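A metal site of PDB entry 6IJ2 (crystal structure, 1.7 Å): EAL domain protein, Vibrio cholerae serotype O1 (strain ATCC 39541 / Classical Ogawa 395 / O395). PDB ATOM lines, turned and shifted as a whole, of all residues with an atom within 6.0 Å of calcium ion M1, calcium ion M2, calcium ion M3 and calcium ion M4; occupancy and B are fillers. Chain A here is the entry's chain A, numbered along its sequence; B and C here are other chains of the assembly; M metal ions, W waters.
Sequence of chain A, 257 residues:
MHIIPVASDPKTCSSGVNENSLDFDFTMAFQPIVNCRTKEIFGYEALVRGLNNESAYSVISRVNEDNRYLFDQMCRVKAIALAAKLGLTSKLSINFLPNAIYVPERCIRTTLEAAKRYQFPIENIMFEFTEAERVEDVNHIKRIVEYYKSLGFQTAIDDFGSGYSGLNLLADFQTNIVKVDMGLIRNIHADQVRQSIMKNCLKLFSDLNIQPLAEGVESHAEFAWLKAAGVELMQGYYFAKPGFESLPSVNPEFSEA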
ATOM      1  N   GLU A  45     -21.909   9.600  18.974  1.00  0.00           N
ATOM      2  CA  GLU A  45     -21.635   9.488  17.559  1.00  0.00           C
ATOM      3  C   GLU A  45     -22.499  10.505  16.812  1.00  0.00           C
ATOM      4  O   GLU A  45     -23.708  10.617  17.084  1.00  0.00           O
ATOM      5  CB  GLU A  45     -21.907   8.075  17.043  1.00  0.00           C
ATOM      6  CG  GLU A  45     -21.642   7.960  15.565  1.00  0.00           C
ATOM      7  CD  GLU A  45     -21.903   6.585  14.994  1.00  0.00           C
ATOM      8  OE1 GLU A  45     -22.477   5.715  15.694  1.00  0.00           O
ATOM      9  OE2 GLU A  45     -21.515   6.397  13.821  1.00  0.00           O
ATOM     10  N   LEU A  47     -24.344  11.737  13.487  1.00  0.00           N
ATOM     11  CA  LEU A  47     -25.010  11.037  12.392  1.00  0.00           C
ATOM     12  C   LEU A  47     -25.733  12.050  11.521  1.00  0.00           C
ATOM     13  O   LEU A  47     -26.501  12.871  12.035  1.00  0.00           O
ATOM     14  CB  LEU A  47     -26.002  10.010  12.920  1.00  0.00           C
ATOM     15  CG  LEU A  47     -25.373   8.895  13.760  1.00  0.00           C
ATOM     16  CD1 LEU A  47     -26.455   8.239  14.581  1.00  0.00           C
ATOM     17  CD2 LEU A  47     -24.686   7.869  12.858  1.00  0.00           C
ATOM     18  N   ASN A  95     -18.081   9.720  11.625  1.00  0.00           N
ATOM     19  CA  ASN A  95     -17.922   8.680  10.612  1.00  0.00           C
ATOM     20  C   ASN A  95     -17.053   9.217   9.479  1.00  0.00           C
ATOM     21  O   ASN A  95     -17.309  10.299   8.945  1.00  0.00           O
ATOM     22  CB  ASN A  95     -19.285   8.261  10.063  1.00  0.00           C
ATOM     23  CG  ASN A  95     -20.088   7.457  11.058  1.00  0.00           C
ATOM     24  OD1 ASN A  95     -19.852   6.270  11.258  1.00  0.00           O
ATOM     25  ND2 ASN A  95     -21.052   8.110  11.703  1.00  0.00           N
ATOM     26  N   GLU A 128     -14.391   7.177  13.058  1.00  0.00           N
ATOM     27  CA  GLU A 128     -14.778   5.792  12.818  1.00  0.00           C
ATOM     28  C   GLU A 128     -14.542   5.452  11.349  1.00  0.00           C
ATOM     29  O   GLU A 128     -15.023   6.163  10.459  1.00  0.00           O
ATOM     30  CB  GLU A 128     -16.240   5.559  13.186  1.00  0.00           C
ATOM     31  CG  GLU A 128     -16.566   6.050  14.581  1.00  0.00           C
ATOM     32  CD  GLU A 128     -17.964   5.697  15.018  1.00  0.00           C
ATOM     33  OE1 GLU A 128     -18.305   6.004  16.173  1.00  0.00           O
ATOM     34  OE2 GLU A 128     -18.726   5.095  14.218  1.00  0.00           O
ATOM     35  N   THR A 130     -14.689   3.073   8.047  1.00  0.00           N
ATOM     36  CA  THR A 130     -15.337   2.047   7.248  1.00  0.00           C
ATOM     37  C   THR A 130     -14.627   1.980   5.898  1.00  0.00           C
ATOM     38  O   THR A 130     -14.312   3.015   5.293  1.00  0.00           O
ATOM     39  CB  THR A 130     -16.828   2.349   7.010  1.00  0.00           C
ATOM     40  OG1 THR A 130     -17.508   2.466   8.268  1.00  0.00           O
ATOM     41  CG2 THR A 130     -17.473   1.236   6.195  1.00  0.00           C
ATOM     42  N   GLU A 131     -14.387   0.764   5.429  1.00  0.00           N
ATOM     43  CA  GLU A 131     -13.729   0.561   4.140  1.00  0.00           C
ATOM     44  C   GLU A 131     -14.675   0.888   2.990  1.00  0.00           C
ATOM     45  O   GLU A 131     -15.889   0.673   3.080  1.00  0.00           O
ATOM     46  CB  GLU A 131     -13.242  -0.878   4.025  1.00  0.00           C
ATOM     47  CG  GLU A 131     -12.485  -1.386   5.255  1.00  0.00           C
ATOM     48  CD  GLU A 131     -13.386  -2.093   6.269  1.00  0.00           C
ATOM     49  OE1 GLU A 131     -14.444  -1.527   6.621  1.00  0.00           O
ATOM     50  OE2 GLU A 131     -13.032  -3.213   6.699  1.00  0.00           O
ATOM     51  N   ILE A 157     -12.337   1.179  14.383  1.00  0.00           N
ATOM     52  CA  ILE A 157     -12.898   0.387  13.294  1.00  0.00           C
ATOM     53  C   ILE A 157     -14.400   0.315  13.512  1.00  0.00           C
ATOM     54  O   ILE A 157     -14.875  -0.123  14.557  1.00  0.00           O
ATOM     55  CB  ILE A 157     -12.259  -1.017  13.239  1.00  0.00           C
ATOM     56  CG1 ILE A 157     -10.785  -0.889  12.878  1.00  0.00           C
ATOM     57  CG2 ILE A 157     -12.996  -1.895  12.232  1.00  0.00           C
ATOM     58  CD1 ILE A 157     -10.060  -2.182  12.862  1.00  0.00           C
ATOM     59  N   ASP A 158     -15.163   0.789  12.522  1.00  0.00           N
ATOM     60  CA  ASP A 158     -16.607   0.972  12.701  1.00  0.00           C
ATOM     61  C   ASP A 158     -17.380  -0.347  12.594  1.00  0.00           C
ATOM     62  O   ASP A 158     -18.316  -0.602  13.363  1.00  0.00           O
ATOM     63  CB  ASP A 158     -17.090   1.979  11.656  1.00  0.00           C
ATOM     64  CG  ASP A 158     -18.463   2.567  11.948  1.00  0.00           C
ATOM     65  OD1 ASP A 158     -19.158   2.131  12.893  1.00  0.00           O
ATOM     66  OD2 ASP A 158     -18.836   3.510  11.233  1.00  0.00           O
ATOM     67  N   ASP A 159     -17.024  -1.198  11.662  1.00  0.00           N
ATOM     68  CA  ASP A 159     -17.980  -2.230  11.292  1.00  0.00           C
ATOM     69  C   ASP A 159     -17.344  -3.593  11.440  1.00  0.00           C
ATOM     70  O   ASP A 159     -17.362  -4.394  10.506  1.00  0.00           O
ATOM     71  CB  ASP A 159     -18.495  -2.025   9.870  1.00  0.00           C
ATOM     72  CG  ASP A 159     -19.141  -0.642   9.661  1.00  0.00           C
ATOM     73  OD1 ASP A 159     -19.496   0.036  10.645  1.00  0.00           O
ATOM     74  OD2 ASP A 159     -19.316  -0.252   8.474  1.00  0.00           O
ATOM     75  N   PHE A 160     -16.786  -3.892  12.603  1.00  0.00           N
ATOM     76  CA  PHE A 160     -16.227  -5.228  12.815  1.00  0.00           C
ATOM     77  C   PHE A 160     -17.345  -6.270  12.868  1.00  0.00           C
ATOM     78  O   PHE A 160     -18.272  -6.175  13.664  1.00  0.00           O
ATOM     79  CB  PHE A 160     -15.423  -5.284  14.096  1.00  0.00           C
ATOM     80  CG  PHE A 160     -14.680  -6.572  14.275  1.00  0.00           C
ATOM     81  CD1 PHE A 160     -13.405  -6.720  13.765  1.00  0.00           C
ATOM     82  CD2 PHE A 160     -15.254  -7.624  14.953  1.00  0.00           C
ATOM     83  CE1 PHE A 160     -12.706  -7.898  13.938  1.00  0.00           C
ATOM     84  CE2 PHE A 160     -14.576  -8.821  15.120  1.00  0.00           C
ATOM     85  CZ  PHE A 160     -13.302  -8.947  14.615  1.00  0.00           C
ATOM     86  N   GLY A 161     -17.221  -7.296  12.049  1.00  0.00           N
ATOM     87  CA  GLY A 161     -18.221  -8.334  12.007  1.00  0.00           C
ATOM     88  C   GLY A 161     -19.282  -8.168  10.947  1.00  0.00           C
ATOM     89  O   GLY A 161     -20.234  -8.959  10.931  1.00  0.00           O
ATOM     90  N   SER A 162     -19.152  -7.187  10.069  1.00  0.00           N
ATOM     91  CA  SER A 162     -20.019  -7.073   8.909  1.00  0.00           C
ATOM     92  C   SER A 162     -19.238  -6.480   7.748  1.00  0.00           C
ATOM     93  O   SER A 162     -18.102  -6.041   7.912  1.00  0.00           O
ATOM     94  CB  SER A 162     -21.239  -6.197   9.204  1.00  0.00           C
ATOM     95  OG  SER A 162     -20.819  -4.868   9.428  1.00  0.00           O
ATOM     96  N   GLY A 163     -19.846  -6.455   6.579  1.00  0.00           N
ATOM     97  CA  GLY A 163     -19.216  -5.776   5.462  1.00  0.00           C
ATOM     98  C   GLY A 163     -17.887  -6.400   5.055  1.00  0.00           C
ATOM     99  O   GLY A 163     -17.814  -7.598   4.729  1.00  0.00           O
ATOM    100  N   TYR A 164     -16.829  -5.601   5.077  1.00  0.00           N
ATOM    101  CA  TYR A 164     -15.488  -6.043   4.725  1.00  0.00           C
ATOM    102  C   TYR A 164     -14.782  -6.632   5.939  1.00  0.00           C
ATOM    103  O   TYR A 164     -15.173  -6.406   7.077  1.00  0.00           O
ATOM    104  CB  TYR A 164     -14.712  -4.874   4.124  1.00  0.00           C
ATOM    105  CG  TYR A 164     -15.404  -4.346   2.872  1.00  0.00           C
ATOM    106  CD1 TYR A 164     -15.375  -5.071   1.702  1.00  0.00           C
ATOM    107  CD2 TYR A 164     -16.109  -3.143   2.891  1.00  0.00           C
ATOM    108  CE1 TYR A 164     -16.007  -4.615   0.555  1.00  0.00           C
ATOM    109  CE2 TYR A 164     -16.742  -2.673   1.743  1.00  0.00           C
ATOM    110  CZ  TYR A 164     -16.700  -3.417   0.579  1.00  0.00           C
ATOM    111  OH  TYR A 164     -17.318  -2.965  -0.563  1.00  0.00           O
ATOM    112  N   SER A 165     -13.726  -7.416   5.685  1.00  0.00           N
ATOM    113  CA  SER A 165     -13.072  -8.175   6.749  1.00  0.00           C
ATOM    114  C   SER A 165     -12.362  -7.241   7.717  1.00  0.00           C
ATOM    115  O   SER A 165     -11.382  -6.584   7.345  1.00  0.00           O
ATOM    116  CB  SER A 165     -12.077  -9.183   6.163  1.00  0.00           C
ATOM    117  OG  SER A 165     -11.305  -9.777   7.216  1.00  0.00           O
ATOM    118  N   GLY A 166     -12.851  -7.202   8.961  1.00  0.00           N
ATOM    119  CA  GLY A 166     -12.180  -6.431   9.991  1.00  0.00           C
ATOM    120  C   GLY A 166     -10.898  -7.067  10.474  1.00  0.00           C
ATOM    121  O   GLY A 166      -9.975  -6.373  10.875  1.00  0.00           O
ATOM    122  N   LYS A 179     -15.549  -1.138  17.051  1.00  0.00           N
ATOM    123  CA  LYS A 179     -16.992  -1.200  17.227  1.00  0.00           C
ATOM    124  C   LYS A 179     -17.504  -2.500  16.614  1.00  0.00           C
ATOM    125  O   LYS A 179     -17.194  -2.803  15.461  1.00  0.00           O
ATOM    126  CB  LYS A 179     -17.679  -0.005  16.562  1.00  0.00           C
ATOM    127  CG  LYS A 179     -17.213   1.299  17.196  1.00  0.00           C
ATOM    128  CD  LYS A 179     -18.377   2.194  17.642  1.00  0.00           C
ATOM    129  CE  LYS A 179     -18.952   2.943  16.527  1.00  0.00           C
ATOM    130  NZ  LYS A 179     -20.036   3.910  16.945  1.00  0.00           N
ATOM    131  N   VAL A 180     -18.277  -3.258  17.383  1.00  0.00           N
ATOM    132  CA  VAL A 180     -18.746  -4.572  16.939  1.00  0.00           C
ATOM    133  C   VAL A 180     -20.143  -4.414  16.384  1.00  0.00           C
ATOM    134  O   VAL A 180     -21.061  -3.964  17.080  1.00  0.00           O
ATOM    135  CB  VAL A 180     -18.714  -5.605  18.084  1.00  0.00           C
ATOM    136  CG1 VAL A 180     -19.253  -6.960  17.570  1.00  0.00           C
ATOM    137  CG2 VAL A 180     -17.299  -5.760  18.595  1.00  0.00           C
ATOM    138  N   ASP A 181     -20.315  -4.854  15.127  1.00  0.00           N
ATOM    139  CA  ASP A 181     -21.565  -4.683  14.407  1.00  0.00           C
ATOM    140  C   ASP A 181     -22.718  -5.327  15.172  1.00  0.00           C
ATOM    141  O   ASP A 181     -22.566  -6.378  15.784  1.00  0.00           O
ATOM    142  CB  ASP A 181     -21.446  -5.302  13.020  1.00  0.00           C
ATOM    143  CG  ASP A 181     -22.706  -5.123  12.205  1.00  0.00           C
ATOM    144  OD1 ASP A 181     -22.932  -4.010  11.709  1.00  0.00           O
ATOM    145  OD2 ASP A 181     -23.471  -6.094  12.059  1.00  0.00           O
ATOM    146  N   GLU A 215     -22.210  -2.292  19.324  1.00  0.00           N
ATOM    147  CA  GLU A 215     -23.192  -1.489  18.604  1.00  0.00           C
ATOM    148  C   GLU A 215     -24.570  -2.144  18.578  1.00  0.00           C
ATOM    149  O   GLU A 215     -24.700  -3.371  18.572  1.00  0.00           O
ATOM    150  CB  GLU A 215     -22.762  -1.231  17.163  1.00  0.00           C
ATOM    151  CG  GLU A 215     -21.461  -0.463  16.976  1.00  0.00           C
ATOM    152  CD  GLU A 215     -21.168  -0.170  15.509  1.00  0.00           C
ATOM    153  OE1 GLU A 215     -20.746   0.955  15.207  1.00  0.00           O
ATOM    154  OE2 GLU A 215     -21.369  -1.052  14.635  1.00  0.00           O
ATOM    155  OP3   G B   1     -22.339   1.505  12.185  1.00  0.00           O
ATOM    156  P     G B   1     -22.856   2.473  11.254  1.00  0.00           P
ATOM    157  OP1   G B   1     -22.302   3.764  11.491  1.00  0.00           O
ATOM    158  OP2   G B   1     -22.658   1.899   9.964  1.00  0.00           O
ATOM    159  O5'   G B   1     -24.401   2.449  11.552  1.00  0.00           O
ATOM    160  C5'   G B   1     -25.035   3.507  12.262  1.00  0.00           C
ATOM    161  C4'   G B   1     -26.535   3.394  12.105  1.00  0.00           C
ATOM    162  O4'   G B   1     -27.056   2.491  13.100  1.00  0.00           O
ATOM    163  C3'   G B   1     -27.337   4.684  12.279  1.00  0.00           C
ATOM    164  O3'   G B   1     -28.286   4.898  11.254  1.00  0.00           O
ATOM    165  C2'   G B   1     -28.077   4.475  13.588  1.00  0.00           C
ATOM    166  O2'   G B   1     -29.344   5.059  13.677  1.00  0.00           O
ATOM    167  C1'   G B   1     -28.267   2.966  13.572  1.00  0.00           C
ATOM    168  N9    G B   1     -28.507   2.409  14.896  1.00  0.00           N
ATOM    169  C8    G B   1     -27.956   2.847  16.086  1.00  0.00           C
ATOM    170  N7    G B   1     -28.338   2.139  17.111  1.00  0.00           N
ATOM    171  C5    G B   1     -29.176   1.179  16.567  1.00  0.00           C
ATOM    172  C6    G B   1     -29.892   0.129  17.196  1.00  0.00           C
ATOM    173  O6    G B   1     -29.936  -0.168  18.381  1.00  0.00           O
ATOM    174  N1    G B   1     -30.633  -0.607  16.286  1.00  0.00           N
ATOM    175  C2    G B   1     -30.668  -0.364  14.932  1.00  0.00           C
ATOM    176  N2    G B   1     -31.414  -1.198  14.212  1.00  0.00           N
ATOM    177  N3    G B   1     -29.998   0.597  14.331  1.00  0.00           N
ATOM    178  C4    G B   1     -29.278   1.325  15.204  1.00  0.00           C
ATOM    179  P     G B   2     -28.297   6.195  10.461  1.00  0.00           P
ATOM    180  OP1   G B   2     -28.078   7.265  11.379  1.00  0.00           O
ATOM    181  OP2   G B   2     -29.480   6.177   9.663  1.00  0.00           O
ATOM    182  O5'   G B   2     -27.062   6.061   9.490  1.00  0.00           O
ATOM    183  C5'   G B   2     -27.131   5.291   8.297  1.00  0.00           C
ATOM    184  C4'   G B   2     -25.756   5.179   7.684  1.00  0.00           C
ATOM    185  O4'   G B   2     -25.250   6.498   7.407  1.00  0.00           O
ATOM    186  C3'   G B   2     -24.703   4.500   8.564  1.00  0.00           C
ATOM    187  O3'   G B   2     -23.895   3.604   7.820  1.00  0.00           O
ATOM    188  C2'   G B   2     -23.820   5.661   9.009  1.00  0.00           C
ATOM    189  O2'   G B   2     -22.480   5.341   9.265  1.00  0.00           O
ATOM    190  C1'   G B   2     -23.923   6.584   7.807  1.00  0.00           C
ATOM    191  N9    G B   2     -23.645   7.960   8.200  1.00  0.00           N
ATOM    192  C8    G B   2     -24.353   8.715   9.088  1.00  0.00           C
ATOM    193  N7    G B   2     -23.829   9.884   9.294  1.00  0.00           N
ATOM    194  C5    G B   2     -22.687   9.890   8.507  1.00  0.00           C
ATOM    195  C6    G B   2     -21.714  10.888   8.318  1.00  0.00           C
ATOM    196  O6    G B   2     -21.631  11.996   8.844  1.00  0.00           O
ATOM    197  N1    G B   2     -20.732  10.479   7.432  1.00  0.00           N
ATOM    198  C2    G B   2     -20.686   9.260   6.811  1.00  0.00           C
ATOM    199  N2    G B   2     -19.659   9.053   5.997  1.00  0.00           N
ATOM    200  N3    G B   2     -21.604   8.330   6.965  1.00  0.00           N
ATOM    201  C4    G B   2     -22.570   8.709   7.821  1.00  0.00           C
ATOM    202  N   SER C 165     -16.333  -9.936   5.309  1.00  0.00           N
ATOM    203  CA  SER C 165     -16.235 -10.388   6.702  1.00  0.00           C
ATOM    204  C   SER C 165     -16.604 -11.866   6.832  1.00  0.00           C
ATOM    205  O   SER C 165     -17.757 -12.241   6.632  1.00  0.00           O
ATOM    206  CB  SER C 165     -17.130  -9.527   7.598  1.00  0.00           C
ATOM    207  OG  SER C 165     -17.235 -10.074   8.917  1.00  0.00           O
HETATM  208 CA    CA M   1     -20.394   4.534  12.782  1.00  0.00          CA
HETATM  209 CA    CA M   2     -20.502   0.221  12.869  1.00  0.00          CA
HETATM  210 CA    CA M   3     -16.212  -4.991   8.451  1.00  0.00          CA
HETATM  211 CA    CA M   4     -20.202   2.025   8.804  1.00  0.00          CA
HETATM  212  O   HOH W   1     -16.629  -3.172   6.778  1.00  0.00           O
HETATM  213  O   HOH W   2     -20.829   3.672   7.185  1.00  0.00           O
HETATM  214  O   HOH W   3     -14.258  -3.824   9.161  1.00  0.00           O
HETATM  215  O   HOH W   4     -21.604   3.453  14.446  1.00  0.00           O
HETATM  216  O   HOH W   5     -21.315  -1.612  11.673  1.00  0.00           O
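Calcium ion M1 is bound by OE2 of Glu 128, water W4, OD1 of Asn 95, OE2 of Glu 45, OD2 of Asp 158, OP1 of G 1 of chain B and OD1 of Asp 158.
Five residues have an atom within 4 Å of calcium ion M1: Glu 45, Asn 95, Glu 128, Asp 158 and G 1 of chain B.
The nearest printed residue that does not touch calcium ion M1 is G 2 of chain B (4.2 Å).
Of the 23 residues printed, 4 come within 4 Å of calcium ion M2.
The nearest printed residue that does not touch calcium ion M2 is Lys 179 (4.7 Å).
Calcium ion M3 is bound by O of Ser 162, at 2.2 Å.
O of Tyr 164 binds calcium ion M3 (2.2 Å).
Calcium ion M3 is bound by water W3, 2.4 Å away.
The backbone carbonyl oxygen (O) of Asp 159 is bound to calcium ion M3, 2.4 Å away.
Calcium ion M3 is bound by water W1 (2.5 Å).
Calcium ion M3 has five donor atoms within binding distance.
Calcium ion M2 is bound by water W5, at 2.3 Å.
Calcium ion M2 is bound by the side-chain carboxylate (OD1) of Asp 158, 2.3 Å away.
OP3 of G 1 of chain B is bound to calcium ion M2 (2.3 Å).
Calcium ion M2 is bound by OE2 of Glu 215, at 2.3 Å.
O of Asp 158 binds calcium ion M2 (2.4 Å).
Calcium ion M2 is bound by the side-chain carboxylate (OD1) of Asp 159 (2.4 Å).
OE1 of Glu 215 is bound to calcium ion M2 (2.5 Å).
Water W4 lies within hydrogen-bond range of OE1 of Glu 45 (2.7 Å) and NZ of Lys 179 (3.0 Å).
Water W1 bridges the side-chain carboxylate of Glu 131 (2.7 Å) and the backbone NH of Tyr 164 (3.0 Å).
Of the 23 residues printed, 3 come within 4 Å of calcium ion M3.
Calcium ion M4 is bound by water W2 (2.4 Å), the side-chain carboxylate (OD2) of Asp 159 (2.5 Å), OP2 of G 1 of chain B (2.7 Å), the side-chain hydroxyl (OG1) of Thr 130 (2.8 Å) and the side-chain carboxylate (OD1) of Asp 159 (2.8 Å).
Calcium ion M4 has five donor atoms within binding distance.
OD1 of Asp 181 sits at hydrogen-bond distance from OG of Ser 162, 3.2 Å away.
The side-chain carboxylate of Glu 128 is in salt-bridge range of the side-chain amino group of Lys 179 (2.8 Å).
The side-chain carboxylate of Glu 215 lies close to the side-chain amino group of Lys 179 (3.5 Å).
O of Val 180 is in hydrogen-bond range of N of Glu 215, at 3.0 Å.
The side-chain amide oxygen of Asn 95 sits close to O2' of G 2 of chain B (3.4 Å).
NZ of Lys 179 lies within salt-bridge range of OE1 of Glu 45.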
